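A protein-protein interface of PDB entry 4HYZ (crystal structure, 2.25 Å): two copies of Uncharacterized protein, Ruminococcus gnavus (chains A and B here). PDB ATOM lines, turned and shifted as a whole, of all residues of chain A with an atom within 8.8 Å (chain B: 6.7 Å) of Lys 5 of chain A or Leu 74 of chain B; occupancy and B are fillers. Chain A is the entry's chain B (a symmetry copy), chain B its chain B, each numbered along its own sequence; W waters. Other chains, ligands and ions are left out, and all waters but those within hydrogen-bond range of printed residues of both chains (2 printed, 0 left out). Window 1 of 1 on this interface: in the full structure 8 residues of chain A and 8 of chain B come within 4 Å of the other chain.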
ATOM      1  N   GLU A   2      -3.157   6.558   5.303  1.00  0.00           N
ATOM      2  CA  GLU A   2      -2.207   5.681   6.010  1.00  0.00           C
ATOM      3  C   GLU A   2      -2.601   5.434   7.463  1.00  0.00           C
ATOM      4  O   GLU A   2      -2.981   6.369   8.140  1.00  0.00           O
ATOM      5  CB  GLU A   2      -0.786   6.302   6.030  1.00  0.00           C
ATOM      6  CG  GLU A   2      -0.014   6.301   4.728  1.00  0.00           C
ATOM      7  CD  GLU A   2       1.205   7.199   4.774  1.00  0.00           C
ATOM      8  OE1 GLU A   2       2.206   6.821   5.428  1.00  0.00           O
ATOM      9  OE2 GLU A   2       1.156   8.290   4.163  1.00  0.00           O
ATOM     10  N   ILE A   3      -2.465   4.205   7.938  1.00  0.00           N
ATOM     11  CA  ILE A   3      -2.589   3.824   9.349  1.00  0.00           C
ATOM     12  C   ILE A   3      -1.159   3.634   9.835  1.00  0.00           C
ATOM     13  O   ILE A   3      -0.378   2.910   9.196  1.00  0.00           O
ATOM     14  CB  ILE A   3      -3.464   2.615   9.660  1.00  0.00           C
ATOM     15  CG1 ILE A   3      -4.822   2.737   8.971  1.00  0.00           C
ATOM     16  CG2 ILE A   3      -3.572   2.429  11.210  1.00  0.00           C
ATOM     17  CD1 ILE A   3      -5.804   3.758   9.605  1.00  0.00           C
ATOM     18  N   LEU A   4      -0.799   4.319  10.912  1.00  0.00           N
ATOM     19  CA  LEU A   4       0.573   4.245  11.378  1.00  0.00           C
ATOM     20  C   LEU A   4       0.646   3.611  12.763  1.00  0.00           C
ATOM     21  O   LEU A   4      -0.265   3.772  13.576  1.00  0.00           O
ATOM     22  CB  LEU A   4       1.194   5.648  11.353  1.00  0.00           C
ATOM     23  CG  LEU A   4       1.042   6.402   9.995  1.00  0.00           C
ATOM     24  CD1 LEU A   4       1.161   7.915  10.174  1.00  0.00           C
ATOM     25  CD2 LEU A   4       2.022   5.884   8.938  1.00  0.00           C
ATOM     26  N   LYS A   5       1.730   2.877  13.010  1.00  0.00           N
ATOM     27  CA  LYS A   5       1.951   2.198  14.292  1.00  0.00           C
ATOM     28  C   LYS A   5       2.883   3.060  15.204  1.00  0.00           C
ATOM     29  O   LYS A   5       3.634   2.555  16.034  1.00  0.00           O
ATOM     30  CB  LYS A   5       2.482   0.787  14.078  1.00  0.00           C
ATOM     31  CG  LYS A   5       1.350  -0.195  13.833  1.00  0.00           C
ATOM     32  CD  LYS A   5       1.892  -1.532  13.361  1.00  0.00           C
ATOM     33  CE  LYS A   5       0.718  -2.410  13.006  1.00  0.00           C
ATOM     34  NZ  LYS A   5       1.150  -3.803  12.703  1.00  0.00           N
ATOM     35  N   GLU A   6       2.747   4.382  15.088  1.00  0.00           N
ATOM     36  CA  GLU A   6       3.418   5.376  15.929  1.00  0.00           C
ATOM     37  C   GLU A   6       2.723   6.687  15.703  1.00  0.00           C
ATOM     38  O   GLU A   6       1.904   6.778  14.782  1.00  0.00           O
ATOM     39  CB  GLU A   6       4.948   5.493  15.623  1.00  0.00           C
ATOM     40  CG  GLU A   6       5.284   5.982  14.214  1.00  0.00           C
ATOM     41  CD  GLU A   6       5.211   4.915  13.145  1.00  0.00           C
ATOM     42  OE1 GLU A   6       5.759   3.810  13.371  1.00  0.00           O
ATOM     43  OE2 GLU A   6       4.602   5.177  12.082  1.00  0.00           O
ATOM     44  N   LEU A   7       3.049   7.719  16.498  1.00  0.00           N
ATOM     45  CA  LEU A   7       2.457   9.020  16.242  1.00  0.00           C
ATOM     46  C   LEU A   7       3.013   9.626  14.950  1.00  0.00           C
ATOM     47  O   LEU A   7       4.205   9.485  14.701  1.00  0.00           O
ATOM     48  CB  LEU A   7       2.732  10.007  17.406  1.00  0.00           C
ATOM     49  CG  LEU A   7       2.051   9.710  18.767  1.00  0.00           C
ATOM     50  CD1 LEU A   7       2.718  10.494  19.879  1.00  0.00           C
ATOM     51  CD2 LEU A   7       0.547   9.949  18.700  1.00  0.00           C
ATOM     52  N   PRO A   8       2.225  10.417  14.201  1.00  0.00           N
ATOM     53  CA  PRO A   8       2.791  11.147  13.055  1.00  0.00           C
ATOM     54  C   PRO A   8       3.744  12.272  13.495  1.00  0.00           C
ATOM     55  O   PRO A   8       3.791  12.624  14.683  1.00  0.00           O
ATOM     56  CB  PRO A   8       1.547  11.764  12.384  1.00  0.00           C
ATOM     57  CG  PRO A   8       0.387  11.052  12.960  1.00  0.00           C
ATOM     58  CD  PRO A   8       0.791  10.718  14.355  1.00  0.00           C
ATOM     59  N   LYS A  13       4.541  12.057  22.479  1.00  0.00           N
ATOM     60  CA  LYS A  13       3.889  11.094  23.390  1.00  0.00           C
ATOM     61  C   LYS A  13       3.391  11.721  24.697  1.00  0.00           C
ATOM     62  O   LYS A  13       2.240  11.514  25.067  1.00  0.00           O
ATOM     63  CB  LYS A  13       4.816   9.928  23.730  1.00  0.00           C
ATOM     64  CG  LYS A  13       5.047   8.988  22.565  1.00  0.00           C
ATOM     65  CD  LYS A  13       5.964   7.872  23.024  1.00  0.00           C
ATOM     66  CE  LYS A  13       6.741   7.219  21.928  1.00  0.00           C
ATOM     67  NZ  LYS A  13       7.819   6.361  22.501  1.00  0.00           N
ATOM     68  N   THR A  72      -0.751   3.166  24.211  1.00  0.00           N
ATOM     69  CA  THR A  72      -0.330   2.622  22.915  1.00  0.00           C
ATOM     70  C   THR A  72      -0.568   3.719  21.906  1.00  0.00           C
ATOM     71  O   THR A  72      -1.704   4.153  21.777  1.00  0.00           O
ATOM     72  CB  THR A  72      -1.078   1.339  22.547  1.00  0.00           C
ATOM     73  OG1 THR A  72      -0.862   0.393  23.568  1.00  0.00           O
ATOM     74  CG2 THR A  72      -0.618   0.776  21.216  1.00  0.00           C
ATOM     75  N   TYR A  73       0.474   4.159  21.197  1.00  0.00           N
ATOM     76  CA  TYR A  73       0.404   5.293  20.254  1.00  0.00           C
ATOM     77  C   TYR A  73       0.303   4.844  18.833  1.00  0.00           C
ATOM     78  O   TYR A  73       0.994   3.928  18.405  1.00  0.00           O
ATOM     79  CB  TYR A  73       1.636   6.216  20.424  1.00  0.00           C
ATOM     80  CG  TYR A  73       1.735   6.761  21.832  1.00  0.00           C
ATOM     81  CD1 TYR A  73       0.993   7.875  22.224  1.00  0.00           C
ATOM     82  CD2 TYR A  73       2.516   6.125  22.793  1.00  0.00           C
ATOM     83  CE1 TYR A  73       1.065   8.372  23.519  1.00  0.00           C
ATOM     84  CE2 TYR A  73       2.576   6.602  24.109  1.00  0.00           C
ATOM     85  CZ  TYR A  73       1.877   7.748  24.451  1.00  0.00           C
ATOM     86  OH  TYR A  73       1.913   8.236  25.723  1.00  0.00           O
ATOM     87  N   LEU A  74      -0.592   5.500  18.094  1.00  0.00           N
ATOM     88  CA  LEU A  74      -0.861   5.191  16.698  1.00  0.00           C
ATOM     89  C   LEU A  74      -1.069   6.476  15.961  1.00  0.00           C
ATOM     90  O   LEU A  74      -1.059   7.554  16.546  1.00  0.00           O
ATOM     91  CB  LEU A  74      -2.108   4.266  16.582  1.00  0.00           C
ATOM     92  CG  LEU A  74      -2.098   2.902  17.298  1.00  0.00           C
ATOM     93  CD1 LEU A  74      -3.516   2.315  17.331  1.00  0.00           C
ATOM     94  CD2 LEU A  74      -1.163   1.896  16.592  1.00  0.00           C
ATOM     95  N   GLY A  75      -1.231   6.379  14.659  1.00  0.00           N
ATOM     96  CA  GLY A  75      -1.442   7.581  13.861  1.00  0.00           C
ATOM     97  C   GLY A  75      -2.196   7.278  12.604  1.00  0.00           C
ATOM     98  O   GLY A  75      -2.461   6.111  12.274  1.00  0.00           O
ATOM     99  N   GLN A  76      -2.577   8.329  11.924  1.00  0.00           N
ATOM    100  CA  GLN A  76      -3.304   8.222  10.664  1.00  0.00           C
ATOM    101  C   GLN A  76      -3.045   9.459   9.808  1.00  0.00           C
ATOM    102  O   GLN A  76      -3.010  10.576  10.322  1.00  0.00           O
ATOM    103  CB  GLN A  76      -4.826   8.079  10.931  1.00  0.00           C
ATOM    104  CG  GLN A  76      -5.627   7.799   9.653  1.00  0.00           C
ATOM    105  CD  GLN A  76      -7.118   7.651   9.833  1.00  0.00           C
ATOM    106  OE1 GLN A  76      -7.674   7.743  10.922  1.00  0.00           O
ATOM    107  NE2 GLN A  76      -7.794   7.399   8.754  1.00  0.00           N
ATOM    108  N   GLY A  85      -3.029   9.228  17.598  1.00  0.00           N
ATOM    109  CA  GLY A  85      -3.942   8.429  18.388  1.00  0.00           C
ATOM    110  C   GLY A  85      -3.308   7.732  19.551  1.00  0.00           C
ATOM    111  O   GLY A  85      -2.100   7.468  19.559  1.00  0.00           O
ATOM    112  N   ILE A  87      -4.389   4.580  22.525  1.00  0.00           N
ATOM    113  CA  ILE A  87      -5.191   3.586  23.205  1.00  0.00           C
ATOM    114  C   ILE A  87      -4.664   3.608  24.634  1.00  0.00           C
ATOM    115  O   ILE A  87      -3.491   3.293  24.863  1.00  0.00           O
ATOM    116  CB  ILE A  87      -5.199   2.187  22.564  1.00  0.00           C
ATOM    117  CG1 ILE A  87      -5.611   2.302  21.084  1.00  0.00           C
ATOM    118  CG2 ILE A  87      -6.184   1.300  23.356  1.00  0.00           C
ATOM    119  CD1 ILE A  87      -5.525   1.060  20.282  1.00  0.00           C
ATOM    120  N   SER A 100      -9.990   4.798  23.166  1.00  0.00           N
ATOM    121  CA  SER A 100      -9.311   5.170  21.919  1.00  0.00           C
ATOM    122  C   SER A 100      -9.644   6.612  21.634  1.00  0.00           C
ATOM    123  O   SER A 100     -10.819   6.933  21.422  1.00  0.00           O
ATOM    124  CB  SER A 100      -9.738   4.292  20.748  1.00  0.00           C
ATOM    125  OG  SER A 100      -9.470   2.943  21.061  1.00  0.00           O
ATOM    126  N   ILE B   3      -1.901  -4.253  24.659  1.00  0.00           N
ATOM    127  CA  ILE B   3      -2.225  -3.785  23.308  1.00  0.00           C
ATOM    128  C   ILE B   3      -0.997  -4.114  22.469  1.00  0.00           C
ATOM    129  O   ILE B   3       0.130  -3.762  22.856  1.00  0.00           O
ATOM    130  CB  ILE B   3      -2.639  -2.325  23.167  1.00  0.00           C
ATOM    131  CG1 ILE B   3      -3.727  -1.969  24.180  1.00  0.00           C
ATOM    132  CG2 ILE B   3      -3.056  -2.036  21.687  1.00  0.00           C
ATOM    133  CD1 ILE B   3      -5.141  -2.524  23.864  1.00  0.00           C
ATOM    134  N   LEU B   4      -1.198  -4.830  21.372  1.00  0.00           N
ATOM    135  CA  LEU B   4      -0.060  -5.245  20.573  1.00  0.00           C
ATOM    136  C   LEU B   4      -0.108  -4.615  19.185  1.00  0.00           C
ATOM    137  O   LEU B   4      -1.186  -4.389  18.635  1.00  0.00           O
ATOM    138  CB  LEU B   4      -0.016  -6.778  20.511  1.00  0.00           C
ATOM    139  CG  LEU B   4      -0.090  -7.488  21.898  1.00  0.00           C
ATOM    140  CD1 LEU B   4      -0.589  -8.927  21.770  1.00  0.00           C
ATOM    141  CD2 LEU B   4       1.242  -7.420  22.649  1.00  0.00           C
ATOM    142  N   LYS B   5       1.071  -4.322  18.638  1.00  0.00           N
ATOM    143  CA  LYS B   5       1.198  -3.713  17.310  1.00  0.00           C
ATOM    144  C   LYS B   5       1.484  -4.812  16.237  1.00  0.00           C
ATOM    145  O   LYS B   5       2.135  -4.580  15.222  1.00  0.00           O
ATOM    146  CB  LYS B   5       2.249  -2.610  17.316  1.00  0.00           C
ATOM    147  CG  LYS B   5       1.661  -1.291  17.788  1.00  0.00           C
ATOM    148  CD  LYS B   5       2.758  -0.274  18.043  1.00  0.00           C
ATOM    149  CE  LYS B   5       2.120   0.958  18.638  1.00  0.00           C
ATOM    150  NZ  LYS B   5       3.097   2.075  18.754  1.00  0.00           N
ATOM    151  N   GLU B   6       0.903  -5.994  16.448  1.00  0.00           N
ATOM    152  CA  GLU B   6       0.926  -7.123  15.516  1.00  0.00           C
ATOM    153  C   GLU B   6      -0.124  -8.094  15.972  1.00  0.00           C
ATOM    154  O   GLU B   6      -0.659  -7.920  17.073  1.00  0.00           O
ATOM    155  CB  GLU B   6       2.328  -7.812  15.433  1.00  0.00           C
ATOM    156  CG  GLU B   6       2.802  -8.459  16.735  1.00  0.00           C
ATOM    157  CD  GLU B   6       3.398  -7.494  17.735  1.00  0.00           C
ATOM    158  OE1 GLU B   6       4.241  -6.660  17.324  1.00  0.00           O
ATOM    159  OE2 GLU B   6       3.023  -7.564  18.928  1.00  0.00           O
ATOM    160  N   LEU B   7      -0.413  -9.134  15.173  1.00  0.00           N
ATOM    161  CA  LEU B   7      -1.360 -10.134  15.633  1.00  0.00           C
ATOM    162  C   LEU B   7      -0.762 -10.965  16.772  1.00  0.00           C
ATOM    163  O   LEU B   7       0.419 -11.287  16.706  1.00  0.00           O
ATOM    164  CB  LEU B   7      -1.769 -11.094  14.487  1.00  0.00           C
ATOM    165  CG  LEU B   7      -2.610 -10.501  13.327  1.00  0.00           C
ATOM    166  CD1 LEU B   7      -2.582 -11.420  12.122  1.00  0.00           C
ATOM    167  CD2 LEU B   7      -4.027 -10.171  13.781  1.00  0.00           C
ATOM    168  N   PRO B   8      -1.571 -11.444  17.732  1.00  0.00           N
ATOM    169  CA  PRO B   8      -1.046 -12.387  18.733  1.00  0.00           C
ATOM    170  C   PRO B   8      -0.720 -13.761  18.124  1.00  0.00           C
ATOM    171  O   PRO B   8      -1.106 -14.048  16.981  1.00  0.00           O
ATOM    172  CB  PRO B   8      -2.219 -12.532  19.724  1.00  0.00           C
ATOM    173  CG  PRO B   8      -3.138 -11.415  19.424  1.00  0.00           C
ATOM    174  CD  PRO B   8      -3.003 -11.186  17.957  1.00  0.00           C
ATOM    175  N   THR B  72      -4.065  -3.127   8.446  1.00  0.00           N
ATOM    176  CA  THR B  72      -3.163  -2.841   9.566  1.00  0.00           C
ATOM    177  C   THR B  72      -3.527  -3.820  10.656  1.00  0.00           C
ATOM    178  O   THR B  72      -4.672  -3.809  11.087  1.00  0.00           O
ATOM    179  CB  THR B  72      -3.265  -1.392  10.047  1.00  0.00           C
ATOM    180  OG1 THR B  72      -2.979  -0.544   8.960  1.00  0.00           O
ATOM    181  CG2 THR B  72      -2.311  -1.104  11.191  1.00  0.00           C
ATOM    182  N   TYR B  73      -2.580  -4.648  11.102  1.00  0.00           N
ATOM    183  CA  TYR B  73      -2.825  -5.721  12.086  1.00  0.00           C
ATOM    184  C   TYR B  73      -2.393  -5.336  13.463  1.00  0.00           C
ATOM    185  O   TYR B  73      -1.329  -4.762  13.659  1.00  0.00           O
ATOM    186  CB  TYR B  73      -2.107  -7.025  11.658  1.00  0.00           C
ATOM    187  CG  TYR B  73      -2.572  -7.497  10.298  1.00  0.00           C
ATOM    188  CD1 TYR B  73      -3.746  -8.237  10.160  1.00  0.00           C
ATOM    189  CD2 TYR B  73      -1.881  -7.149   9.143  1.00  0.00           C
ATOM    190  CE1 TYR B  73      -4.191  -8.662   8.914  1.00  0.00           C
ATOM    191  CE2 TYR B  73      -2.332  -7.550   7.879  1.00  0.00           C
ATOM    192  CZ  TYR B  73      -3.466  -8.337   7.779  1.00  0.00           C
ATOM    193  OH  TYR B  73      -3.934  -8.741   6.563  1.00  0.00           O
ATOM    194  N   LEU B  74      -3.250  -5.650  14.434  1.00  0.00           N
ATOM    195  CA  LEU B  74      -3.028  -5.333  15.836  1.00  0.00           C
ATOM    196  C   LEU B  74      -3.503  -6.485  16.664  1.00  0.00           C
ATOM    197  O   LEU B  74      -4.040  -7.460  16.148  1.00  0.00           O
ATOM    198  CB  LEU B  74      -3.772  -4.020  16.216  1.00  0.00           C
ATOM    199  CG  LEU B  74      -3.439  -2.722  15.454  1.00  0.00           C
ATOM    200  CD1 LEU B  74      -4.499  -1.652  15.749  1.00  0.00           C
ATOM    201  CD2 LEU B  74      -2.054  -2.169  15.853  1.00  0.00           C
ATOM    202  N   GLY B  75      -3.286  -6.398  17.959  1.00  0.00           N
ATOM    203  CA  GLY B  75      -3.719  -7.474  18.842  1.00  0.00           C
ATOM    204  C   GLY B  75      -3.966  -6.976  20.231  1.00  0.00           C
ATOM    205  O   GLY B  75      -3.689  -5.812  20.560  1.00  0.00           O
ATOM    206  N   GLN B  76      -4.524  -7.844  21.036  1.00  0.00           N
ATOM    207  CA  GLN B  76      -4.819  -7.538  22.431  1.00  0.00           C
ATOM    208  C   GLN B  76      -4.831  -8.823  23.254  1.00  0.00           C
ATOM    209  O   GLN B  76      -5.341  -9.847  22.803  1.00  0.00           O
ATOM    210  CB  GLN B  76      -6.195  -6.829  22.548  1.00  0.00           C
ATOM    211  CG  GLN B  76      -6.489  -6.337  23.971  1.00  0.00           C
ATOM    212  CD  GLN B  76      -7.813  -5.640  24.163  1.00  0.00           C
ATOM    213  OE1 GLN B  76      -8.617  -5.466  23.255  1.00  0.00           O
ATOM    214  NE2 GLN B  76      -8.054  -5.208  25.364  1.00  0.00           N
ATOM    215  N   TYR B  83      -6.707 -11.749  21.185  1.00  0.00           N
ATOM    216  CA  TYR B  83      -7.616 -11.164  20.201  1.00  0.00           C
ATOM    217  C   TYR B  83      -6.813 -10.524  19.089  1.00  0.00           C
ATOM    218  O   TYR B  83      -5.868  -9.795  19.353  1.00  0.00           O
ATOM    219  CB  TYR B  83      -8.575 -10.150  20.869  1.00  0.00           C
ATOM    220  CG  TYR B  83      -9.375 -10.791  21.981  1.00  0.00           C
ATOM    221  CD1 TYR B  83     -10.530 -11.523  21.705  1.00  0.00           C
ATOM    222  CD2 TYR B  83      -8.938 -10.733  23.302  1.00  0.00           C
ATOM    223  CE1 TYR B  83     -11.252 -12.138  22.719  1.00  0.00           C
ATOM    224  CE2 TYR B  83      -9.641 -11.357  24.321  1.00  0.00           C
ATOM    225  CZ  TYR B  83     -10.800 -12.056  24.023  1.00  0.00           C
ATOM    226  OH  TYR B  83     -11.489 -12.696  25.011  1.00  0.00           O
ATOM    227  N   GLY B  84      -7.157 -10.864  17.867  1.00  0.00           N
ATOM    228  CA  GLY B  84      -6.465 -10.389  16.679  1.00  0.00           C
ATOM    229  C   GLY B  84      -7.306  -9.339  16.016  1.00  0.00           C
ATOM    230  O   GLY B  84      -8.502  -9.522  15.824  1.00  0.00           O
ATOM    231  N   GLY B  85      -6.685  -8.234  15.707  1.00  0.00           N
ATOM    232  CA  GLY B  85      -7.404  -7.117  15.134  1.00  0.00           C
ATOM    233  C   GLY B  85      -6.871  -6.648  13.816  1.00  0.00           C
ATOM    234  O   GLY B  85      -5.695  -6.848  13.492  1.00  0.00           O
ATOM    235  N   VAL B  86      -7.751  -6.019  13.059  1.00  0.00           N
ATOM    236  CA  VAL B  86      -7.386  -5.488  11.781  1.00  0.00           C
ATOM    237  C   VAL B  86      -8.147  -4.160  11.559  1.00  0.00           C
ATOM    238  O   VAL B  86      -9.329  -4.022  11.896  1.00  0.00           O
ATOM    239  CB  VAL B  86      -7.580  -6.540  10.644  1.00  0.00           C
ATOM    240  CG1 VAL B  86      -9.056  -6.856  10.371  1.00  0.00           C
ATOM    241  CG2 VAL B  86      -6.880  -6.111   9.380  1.00  0.00           C
ATOM    242  N   ILE B  87      -7.420  -3.177  11.058  1.00  0.00           N
ATOM    243  CA  ILE B  87      -7.941  -1.925  10.553  1.00  0.00           C
ATOM    244  C   ILE B  87      -7.836  -2.071   9.041  1.00  0.00           C
ATOM    245  O   ILE B  87      -6.727  -2.200   8.509  1.00  0.00           O
ATOM    246  CB  ILE B  87      -7.270  -0.655  11.106  1.00  0.00           C
ATOM    247  CG1 ILE B  87      -7.310  -0.682  12.646  1.00  0.00           C
ATOM    248  CG2 ILE B  87      -8.022   0.571  10.545  1.00  0.00           C
ATOM    249  CD1 ILE B  87      -6.573   0.399  13.339  1.00  0.00           C
HETATM  250  O   HOH W   1       2.901   2.675  21.676  1.00  0.00           O
HETATM  251  O   HOH W   2       0.020  -4.145   9.957  1.00  0.00           O
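The backbone carbonyl oxygen (O) of Lys 5 of chain B is in hydrogen-bond range of the side-chain amino group (NZ) of Lys 5 of chain A (2.8 Å).
The side-chain amino group (NZ) of Lys 5 of chain B lies within hydrogen-bond range of the backbone carbonyl oxygen (O) of Tyr 73 of chain A (2.8 Å).
NZ of Lys 5 of chain A sits at hydrogen-bond distance from O of Tyr 73 of chain B, at 2.8 Å.
Among the printed residues, merely in contact across the chains: Ile 3 of chain A with Thr 72 of chain B (3.3 Å), Ile 3 of chain A with Ile 87 of chain B (3.995 Å), Lys 5 of chain A with Thr 72 of chain B (3.8 Å), Lys 5 of chain A with Leu 74 of chain B (3.98 Å), Thr 72 of chain A with Ile 3 of chain B (3.3 Å), Thr 72 of chain A with Lys 5 of chain B (3.8 Å), Leu 74 of chain A with Lys 5 of chain B (3.98 Å) and Ile 87 of chain A with Ile 3 of chain B (3.996 Å).
Of the printed residues of chain B, Ile 3 of chain A touches Thr 72 and Ile 87.
Printed residues of chain B within 4 Å of Lys 5 of chain A: Lys 5, Thr 72, Tyr 73 and Leu 74.
Gln 76 of chain A touches none of the printed residues of chain B.
Of the printed residues of chain A, Ile 3 of chain B touches Thr 72 (3.3 Å) and Ile 87 (3.996 Å).
Leu 4 of chain B touches none of the printed residues of chain A.
Printed residues of chain A within 4 Å of Lys 5 of chain B: Lys 5 (2.8 Å), Thr 72 (3.8 Å), Tyr 73 (2.8 Å) and Leu 74 (3.98 Å).
Printed residues of chain A within 4 Å of Leu 74 of chain B: Lys 5.
No residue of chain A comes within 4 Å of Gly 85 of chain B.
The nearest printed residue of chain B that does not touch Lys 5 of chain A is Glu 6 of chain B (4.3 Å).
The nearest printed residue of chain A that does not touch Leu 74 of chain B is Leu 74 of chain A (4.2 Å).
Printed residues of chain A that touch a printed residue of chain B: Ile 3, Lys 5, Thr 72, Tyr 73, Leu 74 and Ile 87.
Among the printed residues, 11 pairs touch across the chains.
Among the printed residues, no Asp or Glu carboxylate lies within 4 Å of a Lys or Arg side-chain nitrogen of the other chain.
The backbone NH (N) of Thr 72 of chain B lies within hydrogen-bond range of the backbone carbonyl oxygen (O) of Ile 87 of chain B, 2.8 Å away.
The backbone carbonyl oxygen (O) of Leu 74 of chain B lies within hydrogen-bond range of the backbone NH (N) of Gly 85 of chain B, 2.8 Å away.
The backbone carbonyl oxygen of Lys 13 of chain A sits at hydrogen-bond distance from the side-chain hydroxyl of Tyr 73 of chain A.
The backbone carbonyl oxygen (O) of Ile 87 of chain A is in hydrogen-bond range of the backbone NH (N) of Thr 72 of chain A (2.8 Å).
The backbone NH (N) of Gly 85 of chain A is in hydrogen-bond range of the backbone carbonyl oxygen (O) of Leu 74 of chain A (2.8 Å).
Ile 3 of chain A touches Thr 72 of chain B, and with the chains exchanged Thr 72 of chain A touches Ile 3 of chain B.
Lys 5 of chain A touches its own counterpart, Lys 5 of chain B.
Lys 5 of chain A touches Tyr 73 of chain B, and with the chains exchanged Tyr 73 of chain A touches Lys 5 of chain B.
Lys 5 of chain A touches Leu 74 of chain B, and with the chains exchanged Leu 74 of chain A touches Lys 5 of chain B.
Of the 11 pairs that touch across the chains among the printed residues, 11 have their exchanged pair printed and touching as well.
Water W2 bridges the backbone NH (N) of Tyr 73 of chain B (2.9 Å) and the side-chain amino group (NZ) of Lys 5 of chain A (3.0 Å).
Water W1 lies within hydrogen-bond range of the backbone NH of Tyr 73 of chain A (2.9 Å) and the side-chain amino group of Lys 5 of chain B (3.0 Å).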
